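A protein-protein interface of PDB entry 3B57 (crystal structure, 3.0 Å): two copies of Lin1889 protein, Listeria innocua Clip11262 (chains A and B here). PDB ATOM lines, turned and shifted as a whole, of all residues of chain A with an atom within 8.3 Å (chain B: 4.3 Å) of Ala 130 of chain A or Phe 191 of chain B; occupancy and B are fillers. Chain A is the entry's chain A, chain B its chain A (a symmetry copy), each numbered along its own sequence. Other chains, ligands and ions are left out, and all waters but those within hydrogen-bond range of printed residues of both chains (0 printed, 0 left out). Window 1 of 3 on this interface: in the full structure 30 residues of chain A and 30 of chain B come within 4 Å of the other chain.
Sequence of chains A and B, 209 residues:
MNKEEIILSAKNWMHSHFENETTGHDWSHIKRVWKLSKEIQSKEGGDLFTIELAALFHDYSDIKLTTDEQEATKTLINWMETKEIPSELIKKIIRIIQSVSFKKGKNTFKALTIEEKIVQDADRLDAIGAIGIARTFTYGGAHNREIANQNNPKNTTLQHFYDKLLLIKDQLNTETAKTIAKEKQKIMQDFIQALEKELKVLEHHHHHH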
ATOM      1  N   ARG A  32     -17.698  20.505  -2.969  1.00  0.00           N
ATOM      2  CA  ARG A  32     -16.691  20.205  -3.998  1.00  0.00           C
ATOM      3  C   ARG A  32     -15.733  21.395  -4.120  1.00  0.00           C
ATOM      4  O   ARG A  32     -14.517  21.217  -4.149  1.00  0.00           O
ATOM      5  CB  ARG A  32     -17.347  19.939  -5.367  1.00  0.00           C
ATOM      6  CG  ARG A  32     -17.356  18.469  -5.816  1.00  0.00           C
ATOM      7  CD  ARG A  32     -18.047  18.292  -7.168  1.00  0.00           C
ATOM      8  NE  ARG A  32     -19.454  17.906  -7.039  1.00  0.00           N
ATOM      9  CZ  ARG A  32     -20.477  18.613  -7.518  1.00  0.00           C
ATOM     10  NH1 ARG A  32     -20.257  19.755  -8.160  1.00  0.00           N
ATOM     11  NH2 ARG A  32     -21.720  18.168  -7.366  1.00  0.00           N
ATOM     12  N   LEU A 125     -13.188  25.488 -11.757  1.00  0.00           N
ATOM     13  CA  LEU A 125     -12.909  24.067 -11.974  1.00  0.00           C
ATOM     14  C   LEU A 125     -14.158  23.179 -11.923  1.00  0.00           C
ATOM     15  O   LEU A 125     -14.254  22.200 -12.670  1.00  0.00           O
ATOM     16  CB  LEU A 125     -11.903  23.550 -10.943  1.00  0.00           C
ATOM     17  CG  LEU A 125     -10.416  23.815 -11.200  1.00  0.00           C
ATOM     18  CD1 LEU A 125      -9.584  23.357 -10.001  1.00  0.00           C
ATOM     19  CD2 LEU A 125      -9.980  23.084 -12.460  1.00  0.00           C
ATOM     20  N   ASP A 126     -15.117  23.512 -11.058  1.00  0.00           N
ATOM     21  CA  ASP A 126     -16.323  22.696 -10.942  1.00  0.00           C
ATOM     22  C   ASP A 126     -17.369  22.984 -12.031  1.00  0.00           C
ATOM     23  O   ASP A 126     -18.462  22.400 -12.026  1.00  0.00           O
ATOM     24  CB  ASP A 126     -16.961  22.887  -9.570  1.00  0.00           C
ATOM     25  CG  ASP A 126     -17.760  21.673  -9.136  1.00  0.00           C
ATOM     26  OD1 ASP A 126     -18.932  21.862  -8.731  1.00  0.00           O
ATOM     27  OD2 ASP A 126     -17.210  20.536  -9.184  1.00  0.00           O
ATOM     28  N   ALA A 127     -17.017  23.868 -12.964  1.00  0.00           N
ATOM     29  CA  ALA A 127     -17.905  24.258 -14.041  1.00  0.00           C
ATOM     30  C   ALA A 127     -17.592  23.498 -15.310  1.00  0.00           C
ATOM     31  O   ALA A 127     -18.418  23.440 -16.219  1.00  0.00           O
ATOM     32  CB  ALA A 127     -17.786  25.760 -14.283  1.00  0.00           C
ATOM     33  N   ILE A 128     -16.397  22.919 -15.365  1.00  0.00           N
ATOM     34  CA  ILE A 128     -15.950  22.167 -16.537  1.00  0.00           C
ATOM     35  C   ILE A 128     -15.776  20.702 -16.178  1.00  0.00           C
ATOM     36  O   ILE A 128     -16.045  20.309 -15.048  1.00  0.00           O
ATOM     37  CB  ILE A 128     -14.596  22.688 -17.067  1.00  0.00           C
ATOM     38  CG1 ILE A 128     -13.489  22.379 -16.047  1.00  0.00           C
ATOM     39  CG2 ILE A 128     -14.694  24.179 -17.332  1.00  0.00           C
ATOM     40  CD1 ILE A 128     -12.139  22.961 -16.373  1.00  0.00           C
ATOM     41  N   GLY A 129     -15.302  19.905 -17.135  1.00  0.00           N
ATOM     42  CA  GLY A 129     -15.118  18.483 -16.905  1.00  0.00           C
ATOM     43  C   GLY A 129     -16.449  17.752 -16.862  1.00  0.00           C
ATOM     44  O   GLY A 129     -17.483  18.315 -17.218  1.00  0.00           O
ATOM     45  N   ALA A 130     -16.445  16.501 -16.416  1.00  0.00           N
ATOM     46  CA  ALA A 130     -17.686  15.739 -16.361  1.00  0.00           C
ATOM     47  C   ALA A 130     -18.786  16.484 -15.601  1.00  0.00           C
ATOM     48  O   ALA A 130     -19.930  16.533 -16.059  1.00  0.00           O
ATOM     49  CB  ALA A 130     -17.436  14.385 -15.729  1.00  0.00           C
ATOM     50  N   ILE A 131     -18.433  17.067 -14.450  1.00  0.00           N
ATOM     51  CA  ILE A 131     -19.380  17.826 -13.610  1.00  0.00           C
ATOM     52  C   ILE A 131     -19.945  18.996 -14.405  1.00  0.00           C
ATOM     53  O   ILE A 131     -21.140  19.309 -14.330  1.00  0.00           O
ATOM     54  CB  ILE A 131     -18.693  18.425 -12.364  1.00  0.00           C
ATOM     55  CG1 ILE A 131     -17.730  17.407 -11.766  1.00  0.00           C
ATOM     56  CG2 ILE A 131     -19.741  18.800 -11.310  1.00  0.00           C
ATOM     57  CD1 ILE A 131     -16.705  18.038 -10.813  1.00  0.00           C
ATOM     58  N   GLY A 132     -19.061  19.651 -15.149  1.00  0.00           N
ATOM     59  CA  GLY A 132     -19.477  20.770 -15.967  1.00  0.00           C
ATOM     60  C   GLY A 132     -20.574  20.314 -16.914  1.00  0.00           C
ATOM     61  O   GLY A 132     -21.680  20.869 -16.907  1.00  0.00           O
ATOM     62  N   ILE A 133     -20.269  19.296 -17.722  1.00  0.00           N
ATOM     63  CA  ILE A 133     -21.234  18.756 -18.675  1.00  0.00           C
ATOM     64  C   ILE A 133     -22.561  18.519 -17.971  1.00  0.00           C
ATOM     65  O   ILE A 133     -23.583  19.099 -18.345  1.00  0.00           O
ATOM     66  CB  ILE A 133     -20.733  17.424 -19.294  1.00  0.00           C
ATOM     67  CG1 ILE A 133     -19.504  17.684 -20.165  1.00  0.00           C
ATOM     68  CG2 ILE A 133     -21.828  16.785 -20.131  1.00  0.00           C
ATOM     69  CD1 ILE A 133     -18.845  16.426 -20.697  1.00  0.00           C
ATOM     70  N   ALA A 134     -22.539  17.682 -16.936  1.00  0.00           N
ATOM     71  CA  ALA A 134     -23.752  17.379 -16.177  1.00  0.00           C
ATOM     72  C   ALA A 134     -24.419  18.644 -15.644  1.00  0.00           C
ATOM     73  O   ALA A 134     -25.633  18.811 -15.760  1.00  0.00           O
ATOM     74  CB  ALA A 134     -23.429  16.447 -15.018  1.00  0.00           C
ATOM     75  N   ARG A 135     -23.632  19.537 -15.058  1.00  0.00           N
ATOM     76  CA  ARG A 135     -24.224  20.745 -14.524  1.00  0.00           C
ATOM     77  C   ARG A 135     -24.820  21.648 -15.590  1.00  0.00           C
ATOM     78  O   ARG A 135     -25.968  22.081 -15.457  1.00  0.00           O
ATOM     79  CB  ARG A 135     -23.206  21.510 -13.688  1.00  0.00           C
ATOM     80  CG  ARG A 135     -23.282  21.160 -12.223  1.00  0.00           C
ATOM     81  CD  ARG A 135     -21.947  21.344 -11.532  1.00  0.00           C
ATOM     82  NE  ARG A 135     -21.476  22.726 -11.502  1.00  0.00           N
ATOM     83  CZ  ARG A 135     -22.052  23.701 -10.811  1.00  0.00           C
ATOM     84  NH1 ARG A 135     -21.525  24.919 -10.855  1.00  0.00           N
ATOM     85  NH2 ARG A 135     -23.146  23.457 -10.085  1.00  0.00           N
ATOM     86  N   THR A 136     -24.065  21.915 -16.652  1.00  0.00           N
ATOM     87  CA  THR A 136     -24.557  22.791 -17.707  1.00  0.00           C
ATOM     88  C   THR A 136     -25.778  22.232 -18.442  1.00  0.00           C
ATOM     89  O   THR A 136     -26.666  22.988 -18.833  1.00  0.00           O
ATOM     90  CB  THR A 136     -23.442  23.137 -18.716  1.00  0.00           C
ATOM     91  OG1 THR A 136     -23.971  24.008 -19.721  1.00  0.00           O
ATOM     92  CG2 THR A 136     -22.894  21.895 -19.368  1.00  0.00           C
ATOM     93  N   PHE A 137     -25.837  20.916 -18.623  1.00  0.00           N
ATOM     94  CA  PHE A 137     -26.996  20.328 -19.277  1.00  0.00           C
ATOM     95  C   PHE A 137     -28.179  20.293 -18.321  1.00  0.00           C
ATOM     96  O   PHE A 137     -29.322  20.354 -18.770  1.00  0.00           O
ATOM     97  CB  PHE A 137     -26.696  18.923 -19.798  1.00  0.00           C
ATOM     98  CG  PHE A 137     -26.068  18.921 -21.145  1.00  0.00           C
ATOM     99  CD1 PHE A 137     -26.755  19.455 -22.234  1.00  0.00           C
ATOM    100  CD2 PHE A 137     -24.755  18.472 -21.315  1.00  0.00           C
ATOM    101  CE1 PHE A 137     -26.142  19.556 -23.478  1.00  0.00           C
ATOM    102  CE2 PHE A 137     -24.113  18.562 -22.553  1.00  0.00           C
ATOM    103  CZ  PHE A 137     -24.806  19.107 -23.643  1.00  0.00           C
ATOM    104  N   PHE A 161     -20.333  25.608 -24.689  1.00  0.00           N
ATOM    105  CA  PHE A 161     -19.043  24.938 -24.541  1.00  0.00           C
ATOM    106  C   PHE A 161     -17.946  25.647 -25.328  1.00  0.00           C
ATOM    107  O   PHE A 161     -16.806  25.726 -24.882  1.00  0.00           O
ATOM    108  CB  PHE A 161     -19.111  23.477 -24.999  1.00  0.00           C
ATOM    109  CG  PHE A 161     -19.731  22.549 -23.988  1.00  0.00           C
ATOM    110  CD1 PHE A 161     -21.099  22.560 -23.758  1.00  0.00           C
ATOM    111  CD2 PHE A 161     -18.941  21.668 -23.259  1.00  0.00           C
ATOM    112  CE1 PHE A 161     -21.663  21.705 -22.817  1.00  0.00           C
ATOM    113  CE2 PHE A 161     -19.507  20.815 -22.320  1.00  0.00           C
ATOM    114  CZ  PHE A 161     -20.863  20.835 -22.100  1.00  0.00           C
ATOM    115  N   GLU A 183      -7.429  16.505 -16.998  1.00  0.00           N
ATOM    116  CA  GLU A 183      -8.350  15.389 -17.212  1.00  0.00           C
ATOM    117  C   GLU A 183      -9.753  15.879 -17.559  1.00  0.00           C
ATOM    118  O   GLU A 183     -10.452  15.267 -18.373  1.00  0.00           O
ATOM    119  CB  GLU A 183      -8.435  14.511 -15.974  1.00  0.00           C
ATOM    120  CG  GLU A 183      -7.184  13.748 -15.692  1.00  0.00           C
ATOM    121  CD  GLU A 183      -7.493  12.328 -15.294  1.00  0.00           C
ATOM    122  OE1 GLU A 183      -8.318  12.148 -14.370  1.00  0.00           O
ATOM    123  OE2 GLU A 183      -6.918  11.397 -15.903  1.00  0.00           O
ATOM    124  N   LYS A 184     -10.161  16.984 -16.941  1.00  0.00           N
ATOM    125  CA  LYS A 184     -11.475  17.547 -17.191  1.00  0.00           C
ATOM    126  C   LYS A 184     -11.582  18.083 -18.613  1.00  0.00           C
ATOM    127  O   LYS A 184     -12.476  17.686 -19.358  1.00  0.00           O
ATOM    128  CB  LYS A 184     -11.778  18.662 -16.189  1.00  0.00           C
ATOM    129  CG  LYS A 184     -11.969  18.178 -14.757  1.00  0.00           C
ATOM    130  CD  LYS A 184     -12.609  19.255 -13.889  1.00  0.00           C
ATOM    131  CE  LYS A 184     -13.079  18.696 -12.558  1.00  0.00           C
ATOM    132  NZ  LYS A 184     -14.243  19.465 -12.009  1.00  0.00           N
ATOM    133  N   GLN A 185     -10.669  18.974 -18.989  1.00  0.00           N
ATOM    134  CA  GLN A 185     -10.673  19.556 -20.330  1.00  0.00           C
ATOM    135  C   GLN A 185     -10.590  18.470 -21.389  1.00  0.00           C
ATOM    136  O   GLN A 185     -10.852  18.724 -22.560  1.00  0.00           O
ATOM    137  CB  GLN A 185      -9.489  20.503 -20.508  1.00  0.00           C
ATOM    138  CG  GLN A 185      -9.410  21.144 -21.888  1.00  0.00           C
ATOM    139  CD  GLN A 185     -10.287  22.376 -22.009  1.00  0.00           C
ATOM    140  OE1 GLN A 185     -10.210  23.115 -22.994  1.00  0.00           O
ATOM    141  NE2 GLN A 185     -11.129  22.609 -21.002  1.00  0.00           N
ATOM    142  N   LYS A 186     -10.207  17.263 -20.989  1.00  0.00           N
ATOM    143  CA  LYS A 186     -10.108  16.189 -21.960  1.00  0.00           C
ATOM    144  C   LYS A 186     -11.459  15.554 -22.207  1.00  0.00           C
ATOM    145  O   LYS A 186     -11.993  15.641 -23.309  1.00  0.00           O
ATOM    146  CB  LYS A 186      -9.122  15.118 -21.502  1.00  0.00           C
ATOM    147  CG  LYS A 186      -9.139  13.857 -22.357  1.00  0.00           C
ATOM    148  CD  LYS A 186      -8.196  12.798 -21.785  1.00  0.00           C
ATOM    149  CE  LYS A 186      -8.258  11.499 -22.589  1.00  0.00           C
ATOM    150  NZ  LYS A 186      -8.217  11.768 -24.067  1.00  0.00           N
ATOM    151  N   ILE A 187     -12.014  14.922 -21.178  1.00  0.00           N
ATOM    152  CA  ILE A 187     -13.309  14.265 -21.300  1.00  0.00           C
ATOM    153  C   ILE A 187     -14.333  15.222 -21.908  1.00  0.00           C
ATOM    154  O   ILE A 187     -15.218  14.823 -22.656  1.00  0.00           O
ATOM    155  CB  ILE A 187     -13.791  13.779 -19.926  1.00  0.00           C
ATOM    156  CG1 ILE A 187     -14.638  12.507 -20.102  1.00  0.00           C
ATOM    157  CG2 ILE A 187     -14.504  14.908 -19.189  1.00  0.00           C
ATOM    158  CD1 ILE A 187     -15.923  12.679 -20.866  1.00  0.00           C
ATOM    159  N   MET A 188     -14.190  16.498 -21.592  1.00  0.00           N
ATOM    160  CA  MET A 188     -15.095  17.497 -22.106  1.00  0.00           C
ATOM    161  C   MET A 188     -14.886  17.594 -23.611  1.00  0.00           C
ATOM    162  O   MET A 188     -15.841  17.652 -24.384  1.00  0.00           O
ATOM    163  CB  MET A 188     -14.802  18.828 -21.430  1.00  0.00           C
ATOM    164  CG  MET A 188     -15.840  19.878 -21.677  1.00  0.00           C
ATOM    165  SD  MET A 188     -15.695  21.332 -20.435  1.00  0.00           S
ATOM    166  CE  MET A 188     -17.270  20.927 -19.414  1.00  0.00           C
ATOM    167  N   GLN A 189     -13.623  17.593 -24.024  1.00  0.00           N
ATOM    168  CA  GLN A 189     -13.286  17.673 -25.437  1.00  0.00           C
ATOM    169  C   GLN A 189     -13.803  16.409 -26.139  1.00  0.00           C
ATOM    170  O   GLN A 189     -14.433  16.489 -27.194  1.00  0.00           O
ATOM    171  CB  GLN A 189     -11.772  17.816 -25.589  1.00  0.00           C
ATOM    172  CG  GLN A 189     -11.361  18.793 -26.677  1.00  0.00           C
ATOM    173  CD  GLN A 189     -10.335  19.814 -26.193  1.00  0.00           C
ATOM    174  OE1 GLN A 189      -9.365  19.457 -25.506  1.00  0.00           O
ATOM    175  NE2 GLN A 189     -10.534  21.089 -26.562  1.00  0.00           N
ATOM    176  N   ASP A 190     -13.552  15.250 -25.540  1.00  0.00           N
ATOM    177  CA  ASP A 190     -14.025  13.997 -26.103  1.00  0.00           C
ATOM    178  C   ASP A 190     -15.538  13.996 -26.178  1.00  0.00           C
ATOM    179  O   ASP A 190     -16.118  13.620 -27.196  1.00  0.00           O
ATOM    180  CB  ASP A 190     -13.552  12.819 -25.265  1.00  0.00           C
ATOM    181  CG  ASP A 190     -12.092  12.516 -25.478  1.00  0.00           C
ATOM    182  OD1 ASP A 190     -11.452  13.243 -26.279  1.00  0.00           O
ATOM    183  OD2 ASP A 190     -11.585  11.559 -24.846  1.00  0.00           O
ATOM    184  N   PHE A 191     -16.180  14.419 -25.097  1.00  0.00           N
ATOM    185  CA  PHE A 191     -17.630  14.464 -25.079  1.00  0.00           C
ATOM    186  C   PHE A 191     -18.135  15.310 -26.247  1.00  0.00           C
ATOM    187  O   PHE A 191     -18.979  14.857 -27.022  1.00  0.00           O
ATOM    188  CB  PHE A 191     -18.132  15.027 -23.750  1.00  0.00           C
ATOM    189  CG  PHE A 191     -19.594  15.323 -23.748  1.00  0.00           C
ATOM    190  CD1 PHE A 191     -20.049  16.638 -23.840  1.00  0.00           C
ATOM    191  CD2 PHE A 191     -20.522  14.292 -23.739  1.00  0.00           C
ATOM    192  CE1 PHE A 191     -21.412  16.925 -23.932  1.00  0.00           C
ATOM    193  CE2 PHE A 191     -21.885  14.567 -23.833  1.00  0.00           C
ATOM    194  CZ  PHE A 191     -22.329  15.892 -23.932  1.00  0.00           C
ATOM    195  N   ILE B 133     -26.398  11.248 -22.726  1.00  0.00           N
ATOM    196  CA  ILE B 133     -25.917  12.054 -21.608  1.00  0.00           C
ATOM    197  C   ILE B 133     -26.616  13.405 -21.621  1.00  0.00           C
ATOM    198  O   ILE B 133     -27.305  13.764 -20.664  1.00  0.00           O
ATOM    199  CB  ILE B 133     -24.382  12.267 -21.683  1.00  0.00           C
ATOM    200  CG1 ILE B 133     -23.660  10.935 -21.478  1.00  0.00           C
ATOM    201  CG2 ILE B 133     -23.933  13.261 -20.626  1.00  0.00           C
ATOM    202  CD1 ILE B 133     -22.159  11.006 -21.682  1.00  0.00           C
ATOM    203  N   PHE B 137     -29.504  14.395 -18.867  1.00  0.00           N
ATOM    204  CA  PHE B 137     -29.209  15.458 -17.919  1.00  0.00           C
ATOM    205  C   PHE B 137     -30.127  16.648 -18.159  1.00  0.00           C
ATOM    206  O   PHE B 137     -30.427  17.379 -17.217  1.00  0.00           O
ATOM    207  CB  PHE B 137     -27.747  15.895 -17.998  1.00  0.00           C
ATOM    208  CG  PHE B 137     -26.840  15.053 -17.175  1.00  0.00           C
ATOM    209  CD1 PHE B 137     -27.012  14.992 -15.793  1.00  0.00           C
ATOM    210  CD2 PHE B 137     -25.872  14.248 -17.783  1.00  0.00           C
ATOM    211  CE1 PHE B 137     -26.241  14.129 -15.021  1.00  0.00           C
ATOM    212  CE2 PHE B 137     -25.082  13.372 -17.032  1.00  0.00           C
ATOM    213  CZ  PHE B 137     -25.266  13.308 -15.644  1.00  0.00           C
ATOM    214  N   ILE B 187     -17.960   6.449 -24.961  1.00  0.00           N
ATOM    215  CA  ILE B 187     -17.923   7.797 -24.410  1.00  0.00           C
ATOM    216  C   ILE B 187     -18.793   7.881 -23.157  1.00  0.00           C
ATOM    217  O   ILE B 187     -18.487   8.599 -22.211  1.00  0.00           O
ATOM    218  CB  ILE B 187     -18.405   8.813 -25.455  1.00  0.00           C
ATOM    219  CG1 ILE B 187     -17.683  10.153 -25.238  1.00  0.00           C
ATOM    220  CG2 ILE B 187     -19.927   8.913 -25.430  1.00  0.00           C
ATOM    221  CD1 ILE B 187     -17.975  10.849 -23.935  1.00  0.00           C
ATOM    222  N   MET B 188     -19.875   7.121 -23.153  1.00  0.00           N
ATOM    223  CA  MET B 188     -20.774   7.113 -22.023  1.00  0.00           C
ATOM    224  C   MET B 188     -20.039   6.497 -20.840  1.00  0.00           C
ATOM    225  O   MET B 188     -20.105   7.001 -19.720  1.00  0.00           O
ATOM    226  CB  MET B 188     -22.009   6.300 -22.378  1.00  0.00           C
ATOM    227  CG  MET B 188     -23.130   6.437 -21.395  1.00  0.00           C
ATOM    228  SD  MET B 188     -24.795   5.818 -22.119  1.00  0.00           S
ATOM    229  CE  MET B 188     -25.618   7.540 -22.322  1.00  0.00           C
ATOM    230  N   GLN B 189     -19.322   5.411 -21.102  1.00  0.00           N
ATOM    231  CA  GLN B 189     -18.566   4.730 -20.063  1.00  0.00           C
ATOM    232  C   GLN B 189     -17.462   5.671 -19.560  1.00  0.00           C
ATOM    233  O   GLN B 189     -17.275   5.834 -18.354  1.00  0.00           O
ATOM    234  CB  GLN B 189     -17.983   3.434 -20.625  1.00  0.00           C
ATOM    235  CG  GLN B 189     -18.048   2.268 -19.655  1.00  0.00           C
ATOM    236  CD  GLN B 189     -18.651   1.014 -20.283  1.00  0.00           C
ATOM    237  OE1 GLN B 189     -18.308   0.649 -21.418  1.00  0.00           O
ATOM    238  NE2 GLN B 189     -19.544   0.339 -19.542  1.00  0.00           N
ATOM    239  N   ASP B 190     -16.748   6.300 -20.489  1.00  0.00           N
ATOM    240  CA  ASP B 190     -15.700   7.237 -20.121  1.00  0.00           C
ATOM    241  C   ASP B 190     -16.284   8.391 -19.332  1.00  0.00           C
ATOM    242  O   ASP B 190     -15.741   8.786 -18.300  1.00  0.00           O
ATOM    243  CB  ASP B 190     -14.996   7.768 -21.361  1.00  0.00           C
ATOM    244  CG  ASP B 190     -14.060   6.755 -21.965  1.00  0.00           C
ATOM    245  OD1 ASP B 190     -13.976   5.630 -21.410  1.00  0.00           O
ATOM    246  OD2 ASP B 190     -13.414   7.078 -22.989  1.00  0.00           O
ATOM    247  N   PHE B 191     -17.395   8.931 -19.814  1.00  0.00           N
ATOM    248  CA  PHE B 191     -18.034  10.033 -19.121  1.00  0.00           C
ATOM    249  C   PHE B 191     -18.335   9.630 -17.677  1.00  0.00           C
ATOM    250  O   PHE B 191     -17.957  10.340 -16.744  1.00  0.00           O
ATOM    251  CB  PHE B 191     -19.314  10.450 -19.841  1.00  0.00           C
ATOM    252  CG  PHE B 191     -20.145  11.414 -19.063  1.00  0.00           C
ATOM    253  CD1 PHE B 191     -21.306  10.987 -18.420  1.00  0.00           C
ATOM    254  CD2 PHE B 191     -19.731  12.727 -18.896  1.00  0.00           C
ATOM    255  CE1 PHE B 191     -22.043  11.854 -17.611  1.00  0.00           C
ATOM    256  CE2 PHE B 191     -20.457  13.601 -18.090  1.00  0.00           C
ATOM    257  CZ  PHE B 191     -21.619  13.158 -17.443  1.00  0.00           C
ATOM    258  N   ILE B 192     -19.001   8.491 -17.488  1.00  0.00           N
ATOM    259  CA  ILE B 192     -19.316   8.026 -16.137  1.00  0.00           C
ATOM    260  C   ILE B 192     -18.071   7.884 -15.256  1.00  0.00           C
ATOM    261  O   ILE B 192     -18.020   8.428 -14.147  1.00  0.00           O
ATOM    262  CB  ILE B 192     -20.088   6.687 -16.154  1.00  0.00           C
ATOM    263  CG1 ILE B 192     -21.494   6.933 -16.676  1.00  0.00           C
ATOM    264  CG2 ILE B 192     -20.181   6.114 -14.743  1.00  0.00           C
ATOM    265  CD1 ILE B 192     -22.209   8.067 -15.939  1.00  0.00           C
ATOM    266  N   GLN B 193     -17.072   7.156 -15.740  1.00  0.00           N
ATOM    267  CA  GLN B 193     -15.858   6.996 -14.967  1.00  0.00           C
ATOM    268  C   GLN B 193     -15.406   8.371 -14.508  1.00  0.00           C
ATOM    269  O   GLN B 193     -15.305   8.628 -13.315  1.00  0.00           O
ATOM    270  CB  GLN B 193     -14.787   6.322 -15.815  1.00  0.00           C
ATOM    271  CG  GLN B 193     -15.198   4.931 -16.242  1.00  0.00           C
ATOM    272  CD  GLN B 193     -14.211   4.284 -17.195  1.00  0.00           C
ATOM    273  OE1 GLN B 193     -13.012   4.225 -16.908  1.00  0.00           O
ATOM    274  NE2 GLN B 193     -14.709   3.788 -18.337  1.00  0.00           N
ATOM    275  N   ALA B 194     -15.184   9.266 -15.462  1.00  0.00           N
ATOM    276  CA  ALA B 194     -14.748  10.620 -15.156  1.00  0.00           C
ATOM    277  C   ALA B 194     -15.676  11.337 -14.174  1.00  0.00           C
ATOM    278  O   ALA B 194     -15.211  12.115 -13.348  1.00  0.00           O
ATOM    279  CB  ALA B 194     -14.626  11.430 -16.443  1.00  0.00           C
ATOM    280  N   LEU B 195     -16.980  11.086 -14.251  1.00  0.00           N
ATOM    281  CA  LEU B 195     -17.898  11.759 -13.336  1.00  0.00           C
ATOM    282  C   LEU B 195     -17.595  11.330 -11.908  1.00  0.00           C
ATOM    283  O   LEU B 195     -17.140  12.134 -11.100  1.00  0.00           O
ATOM    284  CB  LEU B 195     -19.369  11.439 -13.666  1.00  0.00           C
ATOM    285  CG  LEU B 195     -20.422  12.527 -13.342  1.00  0.00           C
ATOM    286  CD1 LEU B 195     -21.814  11.923 -13.179  1.00  0.00           C
ATOM    287  CD2 LEU B 195     -20.029  13.247 -12.081  1.00  0.00           C
ATOM    288  N   GLU B 198     -14.324  12.838 -10.514  1.00  0.00           N
ATOM    289  CA  GLU B 198     -14.245  14.241 -10.124  1.00  0.00           C
ATOM    290  C   GLU B 198     -15.427  14.637  -9.268  1.00  0.00           C
ATOM    291  O   GLU B 198     -15.572  15.795  -8.883  1.00  0.00           O
ATOM    292  CB  GLU B 198     -14.133  15.164 -11.352  1.00  0.00           C
ATOM    293  CG  GLU B 198     -15.153  14.962 -12.447  1.00  0.00           C
ATOM    294  CD  GLU B 198     -14.942  15.915 -13.636  1.00  0.00           C
ATOM    295  OE1 GLU B 198     -15.249  17.126 -13.501  1.00  0.00           O
ATOM    296  OE2 GLU B 198     -14.467  15.457 -14.705  1.00  0.00           O
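The backbone NH (N) of Ile 131 of chain A sits close to the side-chain carboxylate (OE1) of Glu 198 of chain B. The backbone NH (N) of Ala 130 of chain A is in hydrogen-bond range of the side-chain carboxylate (OE2) of Glu 198 of chain B. The side-chain carboxylate (OE1) of Glu 198 of chain B lies within salt-bridge range of the side-chain amino group (NZ) of Lys 184 of chain A (3.0 Å).
NH1 of Arg 32 of chain A is in salt-bridge range of OD1 of Asp 126 of chain A, at 2.6 Å. N of Gly 129 of chain A sits close to SD of Met 188 of chain A. O of Leu 125 of chain A lies within hydrogen-bond range of NZ of Lys 184 of chain A (2.8 Å).
Among the printed residues, merely in contact across the chains: Arg 32 of chain A with Glu 198 of chain B (3.9 Å), Ile 128 of chain A with Glu 198 of chain B (3.6 Å), Gly 129 of chain A with Glu 198 of chain B (3.6 Å), Ala 130 of chain A with Phe 191 of chain B (3.6 Å), Ala 130 of chain A with Ala 194 of chain B (3.8 Å), Ala 130 of chain A with Leu 195 of chain B (3.6 Å), Ala 134 of chain A with Phe 137 of chain B (3.6 Å), Phe 137 of chain A with Phe 137 of chain B (3.5 Å), Ile 187 of chain A with Phe 191 of chain B (3.8 Å), Ile 187 of chain A with Ala 194 of chain B (3.8 Å) and Phe 191 of chain A with Ile 187 of chain B (3.8 Å).
Ala 130 of chain A touches just these residues of chain B: Phe 191 (3.6 Å), Ala 194 (3.8 Å), Leu 195 (3.6 Å) and Glu 198 (2.8 Å). Printed residues of chain A within 4 Å of Phe 191 of chain B: Ala 130 and Ile 187. Of the printed residues of chain B, Arg 32 of chain A touches Glu 198. Of the printed residues of chain B, Phe 191 of chain A touches Ile 187 (3.8 Å). Of the printed residues of chain B, Phe 137 of chain A touches Phe 137. Of the printed residues of chain B, Gly 129 of chain A touches Glu 198 (3.6 Å).
Printed residues of chain B that touch a printed residue of chain A: Phe 137, Ile 187, Phe 191, Ala 194, Leu 195 and Glu 198. Among the printed residues, 14 pairs touch across the chains.
Phe 137 of chain A touches its own counterpart, Phe 137 of chain B. Ile 187 of chain A touches Phe 191 of chain B, and with the chains exchanged Phe 191 of chain A touches Ile 187 of chain B.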
